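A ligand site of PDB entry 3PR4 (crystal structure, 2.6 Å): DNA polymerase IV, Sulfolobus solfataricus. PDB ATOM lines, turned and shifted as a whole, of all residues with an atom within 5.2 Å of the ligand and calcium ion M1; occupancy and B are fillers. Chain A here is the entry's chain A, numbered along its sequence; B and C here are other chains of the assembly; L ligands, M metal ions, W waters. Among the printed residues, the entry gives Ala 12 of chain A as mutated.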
ATOM      1  N   ASP A   7       6.621  29.266  -4.343  1.00  0.00           N
ATOM      2  CA  ASP A   7       5.548  28.317  -4.081  1.00  0.00           C
ATOM      3  C   ASP A   7       4.148  28.980  -4.102  1.00  0.00           C
ATOM      4  O   ASP A   7       3.733  29.588  -3.113  1.00  0.00           O
ATOM      5  CB  ASP A   7       5.819  27.664  -2.736  1.00  0.00           C
ATOM      6  CG  ASP A   7       4.858  26.559  -2.417  1.00  0.00           C
ATOM      7  OD1 ASP A   7       4.948  26.021  -1.306  1.00  0.00           O
ATOM      8  OD2 ASP A   7       4.033  26.187  -3.263  1.00  0.00           O
ATOM      9  N   PHE A   8       3.427  28.847  -5.212  1.00  0.00           N
ATOM     10  CA  PHE A   8       2.122  29.521  -5.378  1.00  0.00           C
ATOM     11  C   PHE A   8       1.171  29.181  -4.226  1.00  0.00           C
ATOM     12  O   PHE A   8       1.092  28.044  -3.826  1.00  0.00           O
ATOM     13  CB  PHE A   8       1.465  29.134  -6.714  1.00  0.00           C
ATOM     14  CG  PHE A   8       2.398  29.192  -7.906  1.00  0.00           C
ATOM     15  CD1 PHE A   8       3.616  29.847  -7.839  1.00  0.00           C
ATOM     16  CD2 PHE A   8       2.032  28.600  -9.104  1.00  0.00           C
ATOM     17  CE1 PHE A   8       4.465  29.897  -8.930  1.00  0.00           C
ATOM     18  CE2 PHE A   8       2.856  28.651 -10.206  1.00  0.00           C
ATOM     19  CZ  PHE A   8       4.080  29.297 -10.120  1.00  0.00           C
ATOM     20  N   ASP A   9       0.460  30.164  -3.708  1.00  0.00           N
ATOM     21  CA  ASP A   9      -0.428  29.938  -2.554  1.00  0.00           C
ATOM     22  C   ASP A   9      -1.704  29.166  -2.933  1.00  0.00           C
ATOM     23  O   ASP A   9      -2.356  29.444  -3.954  1.00  0.00           O
ATOM     24  CB  ASP A   9      -0.783  31.275  -1.866  1.00  0.00           C
ATOM     25  CG  ASP A   9       0.449  32.133  -1.525  1.00  0.00           C
ATOM     26  OD1 ASP A   9       1.440  31.579  -0.989  1.00  0.00           O
ATOM     27  OD2 ASP A   9       0.420  33.356  -1.799  1.00  0.00           O
ATOM     28  N   TYR A  10      -2.034  28.164  -2.096  1.00  0.00           N
ATOM     29  CA  TYR A  10      -3.174  27.286  -2.313  1.00  0.00           C
ATOM     30  C   TYR A  10      -3.627  27.270  -3.782  1.00  0.00           C
ATOM     31  O   TYR A  10      -4.786  27.536  -4.106  1.00  0.00           O
ATOM     32  CB  TYR A  10      -4.315  27.682  -1.367  1.00  0.00           C
ATOM     33  CG  TYR A  10      -4.808  29.100  -1.543  1.00  0.00           C
ATOM     34  CD1 TYR A  10      -5.815  29.405  -2.476  1.00  0.00           C
ATOM     35  CD2 TYR A  10      -4.267  30.149  -0.814  1.00  0.00           C
ATOM     36  CE1 TYR A  10      -6.271  30.714  -2.651  1.00  0.00           C
ATOM     37  CE2 TYR A  10      -4.713  31.477  -0.995  1.00  0.00           C
ATOM     38  CZ  TYR A  10      -5.716  31.746  -1.919  1.00  0.00           C
ATOM     39  OH  TYR A  10      -6.173  33.040  -2.111  1.00  0.00           O
ATOM     40  N   PHE A  11      -2.671  26.928  -4.656  1.00  0.00           N
ATOM     41  CA  PHE A  11      -2.771  27.191  -6.109  1.00  0.00           C
ATOM     42  C   PHE A  11      -4.123  26.965  -6.822  1.00  0.00           C
ATOM     43  O   PHE A  11      -4.640  27.856  -7.493  1.00  0.00           O
ATOM     44  CB  PHE A  11      -1.650  26.465  -6.865  1.00  0.00           C
ATOM     45  CG  PHE A  11      -1.546  26.874  -8.320  1.00  0.00           C
ATOM     46  CD1 PHE A  11      -1.380  28.223  -8.661  1.00  0.00           C
ATOM     47  CD2 PHE A  11      -1.613  25.940  -9.330  1.00  0.00           C
ATOM     48  CE1 PHE A  11      -1.280  28.619 -10.002  1.00  0.00           C
ATOM     49  CE2 PHE A  11      -1.523  26.332 -10.685  1.00  0.00           C
ATOM     50  CZ  PHE A  11      -1.355  27.662 -11.015  1.00  0.00           C
ATOM     51  N   ALA A  12      -4.675  25.765  -6.738  1.00  0.00           N
ATOM     52  CA  ALA A  12      -5.843  25.438  -7.538  1.00  0.00           C
ATOM     53  C   ALA A  12      -7.013  26.355  -7.158  1.00  0.00           C
ATOM     54  O   ALA A  12      -7.688  26.901  -8.027  1.00  0.00           O
ATOM     55  CB  ALA A  12      -6.234  23.988  -7.373  1.00  0.00           C
ATOM     56  N   ALA A  13      -7.230  26.522  -5.863  1.00  0.00           N
ATOM     57  CA  ALA A  13      -8.273  27.392  -5.367  1.00  0.00           C
ATOM     58  C   ALA A  13      -8.033  28.839  -5.753  1.00  0.00           C
ATOM     59  O   ALA A  13      -8.927  29.481  -6.295  1.00  0.00           O
ATOM     60  CB  ALA A  13      -8.416  27.240  -3.884  1.00  0.00           C
ATOM     61  N   VAL A  43     -10.689  15.810  -1.269  1.00  0.00           N
ATOM     62  CA  VAL A  43     -10.306  17.206  -1.434  1.00  0.00           C
ATOM     63  C   VAL A  43      -8.936  17.259  -2.109  1.00  0.00           C
ATOM     64  O   VAL A  43      -8.004  16.554  -1.710  1.00  0.00           O
ATOM     65  CB  VAL A  43     -10.276  17.945  -0.081  1.00  0.00           C
ATOM     66  CG1 VAL A  43     -10.070  19.466  -0.279  1.00  0.00           C
ATOM     67  CG2 VAL A  43     -11.552  17.663   0.671  1.00  0.00           C
ATOM     68  N   ALA A  44      -8.795  18.082  -3.138  1.00  0.00           N
ATOM     69  CA  ALA A  44      -7.499  18.243  -3.781  1.00  0.00           C
ATOM     70  C   ALA A  44      -6.779  19.371  -3.090  1.00  0.00           C
ATOM     71  O   ALA A  44      -5.642  19.227  -2.695  1.00  0.00           O
ATOM     72  CB  ALA A  44      -7.645  18.515  -5.271  1.00  0.00           C
ATOM     73  N   THR A  45      -7.455  20.505  -2.964  1.00  0.00           N
ATOM     74  CA  THR A  45      -6.941  21.635  -2.205  1.00  0.00           C
ATOM     75  C   THR A  45      -8.086  22.551  -1.777  1.00  0.00           C
ATOM     76  O   THR A  45      -9.148  22.603  -2.418  1.00  0.00           O
ATOM     77  CB  THR A  45      -5.863  22.437  -2.978  1.00  0.00           C
ATOM     78  OG1 THR A  45      -5.558  23.621  -2.252  1.00  0.00           O
ATOM     79  CG2 THR A  45      -6.382  22.871  -4.314  1.00  0.00           C
ATOM     80  N   TYR A  48      -7.497  29.109   2.358  1.00  0.00           N
ATOM     81  CA  TYR A  48      -7.220  29.168   3.789  1.00  0.00           C
ATOM     82  C   TYR A  48      -8.462  29.338   4.691  1.00  0.00           C
ATOM     83  O   TYR A  48      -8.490  28.790   5.792  1.00  0.00           O
ATOM     84  CB  TYR A  48      -6.105  30.173   4.085  1.00  0.00           C
ATOM     85  CG  TYR A  48      -4.728  29.590   3.775  1.00  0.00           C
ATOM     86  CD1 TYR A  48      -4.317  29.372   2.457  1.00  0.00           C
ATOM     87  CD2 TYR A  48      -3.856  29.228   4.800  1.00  0.00           C
ATOM     88  CE1 TYR A  48      -3.079  28.834   2.183  1.00  0.00           C
ATOM     89  CE2 TYR A  48      -2.613  28.684   4.533  1.00  0.00           C
ATOM     90  CZ  TYR A  48      -2.230  28.486   3.228  1.00  0.00           C
ATOM     91  OH  TYR A  48      -0.990  27.929   2.966  1.00  0.00           O
ATOM     92  N   ARG A  51      -9.196  25.915   4.944  1.00  0.00           N
ATOM     93  CA  ARG A  51      -8.163  25.242   5.732  1.00  0.00           C
ATOM     94  C   ARG A  51      -8.311  25.545   7.227  1.00  0.00           C
ATOM     95  O   ARG A  51      -8.133  24.675   8.054  1.00  0.00           O
ATOM     96  CB  ARG A  51      -6.751  25.593   5.256  1.00  0.00           C
ATOM     97  CG  ARG A  51      -6.266  24.849   3.994  1.00  0.00           C
ATOM     98  CD  ARG A  51      -4.785  25.128   3.743  1.00  0.00           C
ATOM     99  NE  ARG A  51      -4.220  24.364   2.635  1.00  0.00           N
ATOM    100  CZ  ARG A  51      -3.821  24.898   1.482  1.00  0.00           C
ATOM    101  NH1 ARG A  51      -3.935  26.211   1.283  1.00  0.00           N
ATOM    102  NH2 ARG A  51      -3.316  24.128   0.510  1.00  0.00           N
ATOM    103  N   ALA A  57      -6.284  19.215   1.961  1.00  0.00           N
ATOM    104  CA  ALA A  57      -6.023  18.207   0.938  1.00  0.00           C
ATOM    105  C   ALA A  57      -6.062  16.810   1.516  1.00  0.00           C
ATOM    106  O   ALA A  57      -5.480  16.522   2.572  1.00  0.00           O
ATOM    107  CB  ALA A  57      -4.677  18.465   0.289  1.00  0.00           C
ATOM    108  N   GLY A  58      -6.759  15.924   0.816  1.00  0.00           N
ATOM    109  CA  GLY A  58      -6.679  14.508   1.140  1.00  0.00           C
ATOM    110  C   GLY A  58      -7.854  13.876   1.842  1.00  0.00           C
ATOM    111  O   GLY A  58      -8.024  12.664   1.759  1.00  0.00           O
ATOM    112  N   MET A  76     -12.026  19.750  -9.583  1.00  0.00           N
ATOM    113  CA  MET A  76     -10.712  19.998 -10.107  1.00  0.00           C
ATOM    114  C   MET A  76     -10.741  20.317 -11.596  1.00  0.00           C
ATOM    115  O   MET A  76     -11.404  19.614 -12.367  1.00  0.00           O
ATOM    116  CB  MET A  76      -9.872  18.754  -9.887  1.00  0.00           C
ATOM    117  CG  MET A  76      -8.402  19.028  -9.849  1.00  0.00           C
ATOM    118  SD  MET A  76      -7.920  19.905  -8.376  1.00  0.00           S
ATOM    119  CE  MET A  76      -6.153  19.697  -8.452  1.00  0.00           C
ATOM    120  N   ILE A 104       3.775  21.560 -10.507  1.00  0.00           N
ATOM    121  CA  ILE A 104       2.897  22.533 -11.109  1.00  0.00           C
ATOM    122  C   ILE A 104       2.982  23.913 -10.437  1.00  0.00           C
ATOM    123  O   ILE A 104       2.613  24.924 -11.034  1.00  0.00           O
ATOM    124  CB  ILE A 104       1.452  22.083 -11.018  1.00  0.00           C
ATOM    125  CG1 ILE A 104       0.627  22.787 -12.084  1.00  0.00           C
ATOM    126  CG2 ILE A 104       0.905  22.293  -9.585  1.00  0.00           C
ATOM    127  CD1 ILE A 104      -0.793  22.624 -11.917  1.00  0.00           C
ATOM    128  N   ASP A 105       3.450  23.976  -9.193  1.00  0.00           N
ATOM    129  CA  ASP A 105       3.440  25.266  -8.537  1.00  0.00           C
ATOM    130  C   ASP A 105       4.675  25.508  -7.700  1.00  0.00           C
ATOM    131  O   ASP A 105       4.620  26.195  -6.683  1.00  0.00           O
ATOM    132  CB  ASP A 105       2.190  25.430  -7.671  1.00  0.00           C
ATOM    133  CG  ASP A 105       2.230  24.555  -6.439  1.00  0.00           C
ATOM    134  OD1 ASP A 105       2.819  23.466  -6.469  1.00  0.00           O
ATOM    135  OD2 ASP A 105       1.660  24.958  -5.421  1.00  0.00           O
ATOM    136  N   LYS A 159       4.429  30.877   4.514  1.00  0.00           N
ATOM    137  CA  LYS A 159       3.234  30.920   3.665  1.00  0.00           C
ATOM    138  C   LYS A 159       1.982  31.088   4.503  1.00  0.00           C
ATOM    139  O   LYS A 159       1.920  30.581   5.629  1.00  0.00           O
ATOM    140  CB  LYS A 159       3.132  29.693   2.758  1.00  0.00           C
ATOM    141  CG  LYS A 159       2.994  28.339   3.477  1.00  0.00           C
ATOM    142  CD  LYS A 159       2.497  27.237   2.541  1.00  0.00           C
ATOM    143  CE  LYS A 159       3.629  26.643   1.695  1.00  0.00           C
ATOM    144  NZ  LYS A 159       3.351  25.216   1.304  1.00  0.00           N
ATOM    145  P    DT B   5      -9.848   7.275  -3.369  1.00  0.00           P
ATOM    146  OP1  DT B   5     -11.234   6.800  -3.627  1.00  0.00           O
ATOM    147  OP2  DT B   5      -8.708   6.346  -3.489  1.00  0.00           O
ATOM    148  O5'  DT B   5      -9.627   8.526  -4.336  1.00  0.00           O
ATOM    149  C5'  DT B   5     -10.698   9.436  -4.479  1.00  0.00           C
ATOM    150  C4'  DT B   5     -10.418  10.326  -5.666  1.00  0.00           C
ATOM    151  O4'  DT B   5      -9.652  11.480  -5.235  1.00  0.00           O
ATOM    152  C3'  DT B   5      -9.578   9.634  -6.730  1.00  0.00           C
ATOM    153  O3'  DT B   5     -10.013  10.075  -8.010  1.00  0.00           O
ATOM    154  C2'  DT B   5      -8.137  10.072  -6.405  1.00  0.00           C
ATOM    155  C1'  DT B   5      -8.336  11.438  -5.738  1.00  0.00           C
ATOM    156  N1   DT B   5      -7.436  11.761  -4.591  1.00  0.00           N
ATOM    157  C2   DT B   5      -6.592  12.853  -4.674  1.00  0.00           C
ATOM    158  O2   DT B   5      -6.522  13.588  -5.651  1.00  0.00           O
ATOM    159  N3   DT B   5      -5.828  13.074  -3.556  1.00  0.00           N
ATOM    160  C4   DT B   5      -5.808  12.321  -2.398  1.00  0.00           C
ATOM    161  O4   DT B   5      -5.063  12.616  -1.460  1.00  0.00           O
ATOM    162  C5   DT B   5      -6.722  11.189  -2.384  1.00  0.00           C
ATOM    163  C7   DT B   5      -6.811  10.300  -1.176  1.00  0.00           C
ATOM    164  C6   DT B   5      -7.479  10.975  -3.466  1.00  0.00           C
ATOM    165  P    DG B   6      -9.675   9.213  -9.308  1.00  0.00           P
ATOM    166  OP1  DG B   6     -10.703   9.496 -10.335  1.00  0.00           O
ATOM    167  OP2  DG B   6      -9.366   7.829  -8.854  1.00  0.00           O
ATOM    168  O5'  DG B   6      -8.335   9.862  -9.839  1.00  0.00           O
ATOM    169  C5'  DG B   6      -8.360  11.225 -10.150  1.00  0.00           C
ATOM    170  C4'  DG B   6      -6.951  11.720 -10.050  1.00  0.00           C
ATOM    171  O4'  DG B   6      -6.495  11.556  -8.702  1.00  0.00           O
ATOM    172  C3'  DG B   6      -5.956  10.897 -10.857  1.00  0.00           C
ATOM    173  O3'  DG B   6      -5.655  11.697 -11.987  1.00  0.00           O
ATOM    174  C2'  DG B   6      -4.764  10.680  -9.903  1.00  0.00           C
ATOM    175  C1'  DG B   6      -5.104  11.690  -8.806  1.00  0.00           C
ATOM    176  N9   DG B   6      -4.546  11.528  -7.476  1.00  0.00           N
ATOM    177  C8   DG B   6      -4.830  10.580  -6.514  1.00  0.00           C
ATOM    178  N7   DG B   6      -4.162  10.762  -5.405  1.00  0.00           N
ATOM    179  C5   DG B   6      -3.393  11.899  -5.653  1.00  0.00           C
ATOM    180  C6   DG B   6      -2.449  12.586  -4.838  1.00  0.00           C
ATOM    181  O6   DG B   6      -2.092  12.325  -3.687  1.00  0.00           O
ATOM    182  N1   DG B   6      -1.909  13.694  -5.496  1.00  0.00           N
ATOM    183  C2   DG B   6      -2.233  14.075  -6.769  1.00  0.00           C
ATOM    184  N2   DG B   6      -1.629  15.165  -7.257  1.00  0.00           N
ATOM    185  N3   DG B   6      -3.111  13.449  -7.540  1.00  0.00           N
ATOM    186  C4   DG B   6      -3.638  12.375  -6.906  1.00  0.00           C
ATOM    187  P    DC C  13       5.115  19.336  -0.597  1.00  0.00           P
ATOM    188  OP1  DC C  13       6.062  20.457  -0.422  1.00  0.00           O
ATOM    189  OP2  DC C  13       4.351  18.923   0.602  1.00  0.00           O
ATOM    190  O5'  DC C  13       4.129  19.650  -1.840  1.00  0.00           O
ATOM    191  C5'  DC C  13       4.722  19.716  -3.157  1.00  0.00           C
ATOM    192  C4'  DC C  13       3.829  19.384  -4.357  1.00  0.00           C
ATOM    193  O4'  DC C  13       3.309  18.033  -4.227  1.00  0.00           O
ATOM    194  C3'  DC C  13       2.597  20.271  -4.593  1.00  0.00           C
ATOM    195  C2'  DC C  13       1.472  19.495  -3.889  1.00  0.00           C
ATOM    196  C1'  DC C  13       1.887  18.099  -4.363  1.00  0.00           C
ATOM    197  N1   DC C  13       1.279  16.901  -3.674  1.00  0.00           N
ATOM    198  C2   DC C  13       0.465  16.066  -4.440  1.00  0.00           C
ATOM    199  O2   DC C  13       0.256  16.352  -5.626  1.00  0.00           O
ATOM    200  N3   DC C  13      -0.079  14.965  -3.860  1.00  0.00           N
ATOM    201  C4   DC C  13       0.175  14.702  -2.583  1.00  0.00           C
ATOM    202  N4   DC C  13      -0.379  13.599  -2.066  1.00  0.00           N
ATOM    203  C5   DC C  13       1.020  15.530  -1.800  1.00  0.00           C
ATOM    204  C6   DC C  13       1.541  16.613  -2.380  1.00  0.00           C
HETATM  205  P1  LIG L   1       0.320  24.101  -0.229  1.00  0.00           P
HETATM  206  O1  LIG L   1       1.297  24.631  -1.276  1.00  0.00           O
HETATM  207  O2  LIG L   1       0.778  23.183   0.926  1.00  0.00           O
HETATM  208  O3  LIG L   1      -0.480  25.353   0.447  1.00  0.00           O
HETATM  209  P2  LIG L   1      -1.228  23.938  -2.537  1.00  0.00           P
HETATM  210  O4  LIG L   1      -2.729  23.957  -2.282  1.00  0.00           O
HETATM  211  O5  LIG L   1      -0.665  25.303  -2.885  1.00  0.00           O
HETATM  212  O6  LIG L   1      -0.709  23.264  -1.158  1.00  0.00           O
HETATM  213  O7  LIG L   1      -0.792  22.775  -3.561  1.00  0.00           O
HETATM  214  C1  LIG L   1      -0.382  23.056  -4.889  1.00  0.00           C
HETATM  215  C2  LIG L   1      -1.266  22.182  -5.797  1.00  0.00           C
HETATM  216  O8  LIG L   1      -1.089  20.789  -5.516  1.00  0.00           O
HETATM  217  C3  LIG L   1      -2.719  22.460  -5.466  1.00  0.00           C
HETATM  218  O9  LIG L   1      -3.269  23.378  -6.395  1.00  0.00           O
HETATM  219  C4  LIG L   1      -3.440  21.119  -5.513  1.00  0.00           C
HETATM  220  C5  LIG L   1      -2.332  20.086  -5.616  1.00  0.00           C
HETATM  221  N1  LIG L   1      -2.407  19.068  -4.515  1.00  0.00           N
HETATM  222  C6  LIG L   1      -1.769  19.143  -3.325  1.00  0.00           C
HETATM  223  N2  LIG L   1      -2.044  18.056  -2.565  1.00  0.00           N
HETATM  224  C7  LIG L   1      -2.871  17.237  -3.248  1.00  0.00           C
HETATM  225  C8  LIG L   1      -3.531  15.931  -3.009  1.00  0.00           C
HETATM  226  N3  LIG L   1      -3.359  15.243  -1.844  1.00  0.00           N
HETATM  227  N4  LIG L   1      -4.322  15.454  -3.990  1.00  0.00           N
HETATM  228  C9  LIG L   1      -4.513  16.101  -5.166  1.00  0.00           C
HETATM  229  N5  LIG L   1      -3.923  17.287  -5.444  1.00  0.00           N
HETATM  230  C10 LIG L   1      -3.101  17.902  -4.546  1.00  0.00           C
HETATM  231 CA    CA M   1       1.661  25.839  -3.237  1.00  0.00          CA
HETATM  232 CA    CA M   2       4.379  23.163  -1.585  1.00  0.00          CA
HETATM  233  O   HOH W   1       3.644  21.773   1.342  1.00  0.00           O
HETATM  234  O   HOH W   2       0.714  21.358  -1.644  1.00  0.00           O
HETATM  235  O   HOH W   3      -0.991  20.932   0.417  1.00  0.00           O
HETATM  236  O   HOH W   4       2.339  23.151  -3.676  1.00  0.00           O
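NH2 of Arg 51 is in salt-bridge range of O4 of the ligand (2.9 Å). O4 of DT 5 of chain B sits at hydrogen-bond distance from a nitrogen (N3) of the ligand (3.2 Å). A nitrogen (N3) of the ligand sits at hydrogen-bond distance from N4 of DC 13 of chain C, at 3.4 Å. The backbone NH (N) of Ala 12 sits at hydrogen-bond distance from an oxygen (O9) of the ligand, at 2.8 Å. The backbone NH (N) of Tyr 10 lies close to an oxygen (O5) of the ligand (3.3 Å). The side-chain hydroxyl of Thr 45 sits at hydrogen-bond distance from an oxygen (O4) of the ligand, at 2.8 Å. The side-chain amino group (NZ) of Lys 159 is in salt-bridge range of an oxygen (O2) of the ligand (3.3 Å). An oxygen (O5) of the ligand lies close to the backbone NH of Phe 11.
Three residues have an atom within 4 Å of calcium ion M1: Asp 7, Phe 8 and Asp 105.
N4 of the ligand lies close to N1 of DG 6 of chain B, 3.3 Å away. Ala 44 touches the ligand. Tyr 48 touches the ligand. Ala 57 touches the ligand. Hydrophobic or aromatic side chains that line the ligand: Phe 11, Ala 12, Ala 44 and Ala 57. Within 4 Å of the ligand: Asp 7, Phe 8, Tyr 10, Phe 11, Ala 12, Ala 44, Thr 45, Tyr 48, Arg 51, Ala 57, Asp 105, Lys 159, DT 5 of chain B, DG 6 of chain B and DC 13 of chain C. The nearest printed residue that does not touch the ligand is Asp 9 (4.001 Å).
Water W4 lies within hydrogen-bond range of OD1 of Asp 105 (2.9 Å) and O7 of the ligand (3.2 Å). Water W1 lies within hydrogen-bond range of OP2 of DC 13 of chain C (3.0 Å), an oxygen (O2) of the ligand (3.2 Å) and the side-chain amino group (NZ) of Lys 159 (3.5 Å).
O1 of the ligand is bound to calcium ion M1 (2.3 Å). O of Phe 8 binds calcium ion M1 (2.4 Å). OD2 of Asp 105 binds calcium ion M1, 2.4 Å away. Calcium ion M1 is bound by OD2 of Asp 7, 2.4 Å away. O5 of the ligand binds calcium ion M1, at 2.4 Å. Water W4 binds calcium ion M1, at 2.8 Å.
OD1 of Asp 7 lies within salt-bridge range of NZ of Lys 159, 3.2 Å away. N4 of DC 13 of chain C sits close to O6 of DG 6 of chain B, at 2.7 Å.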
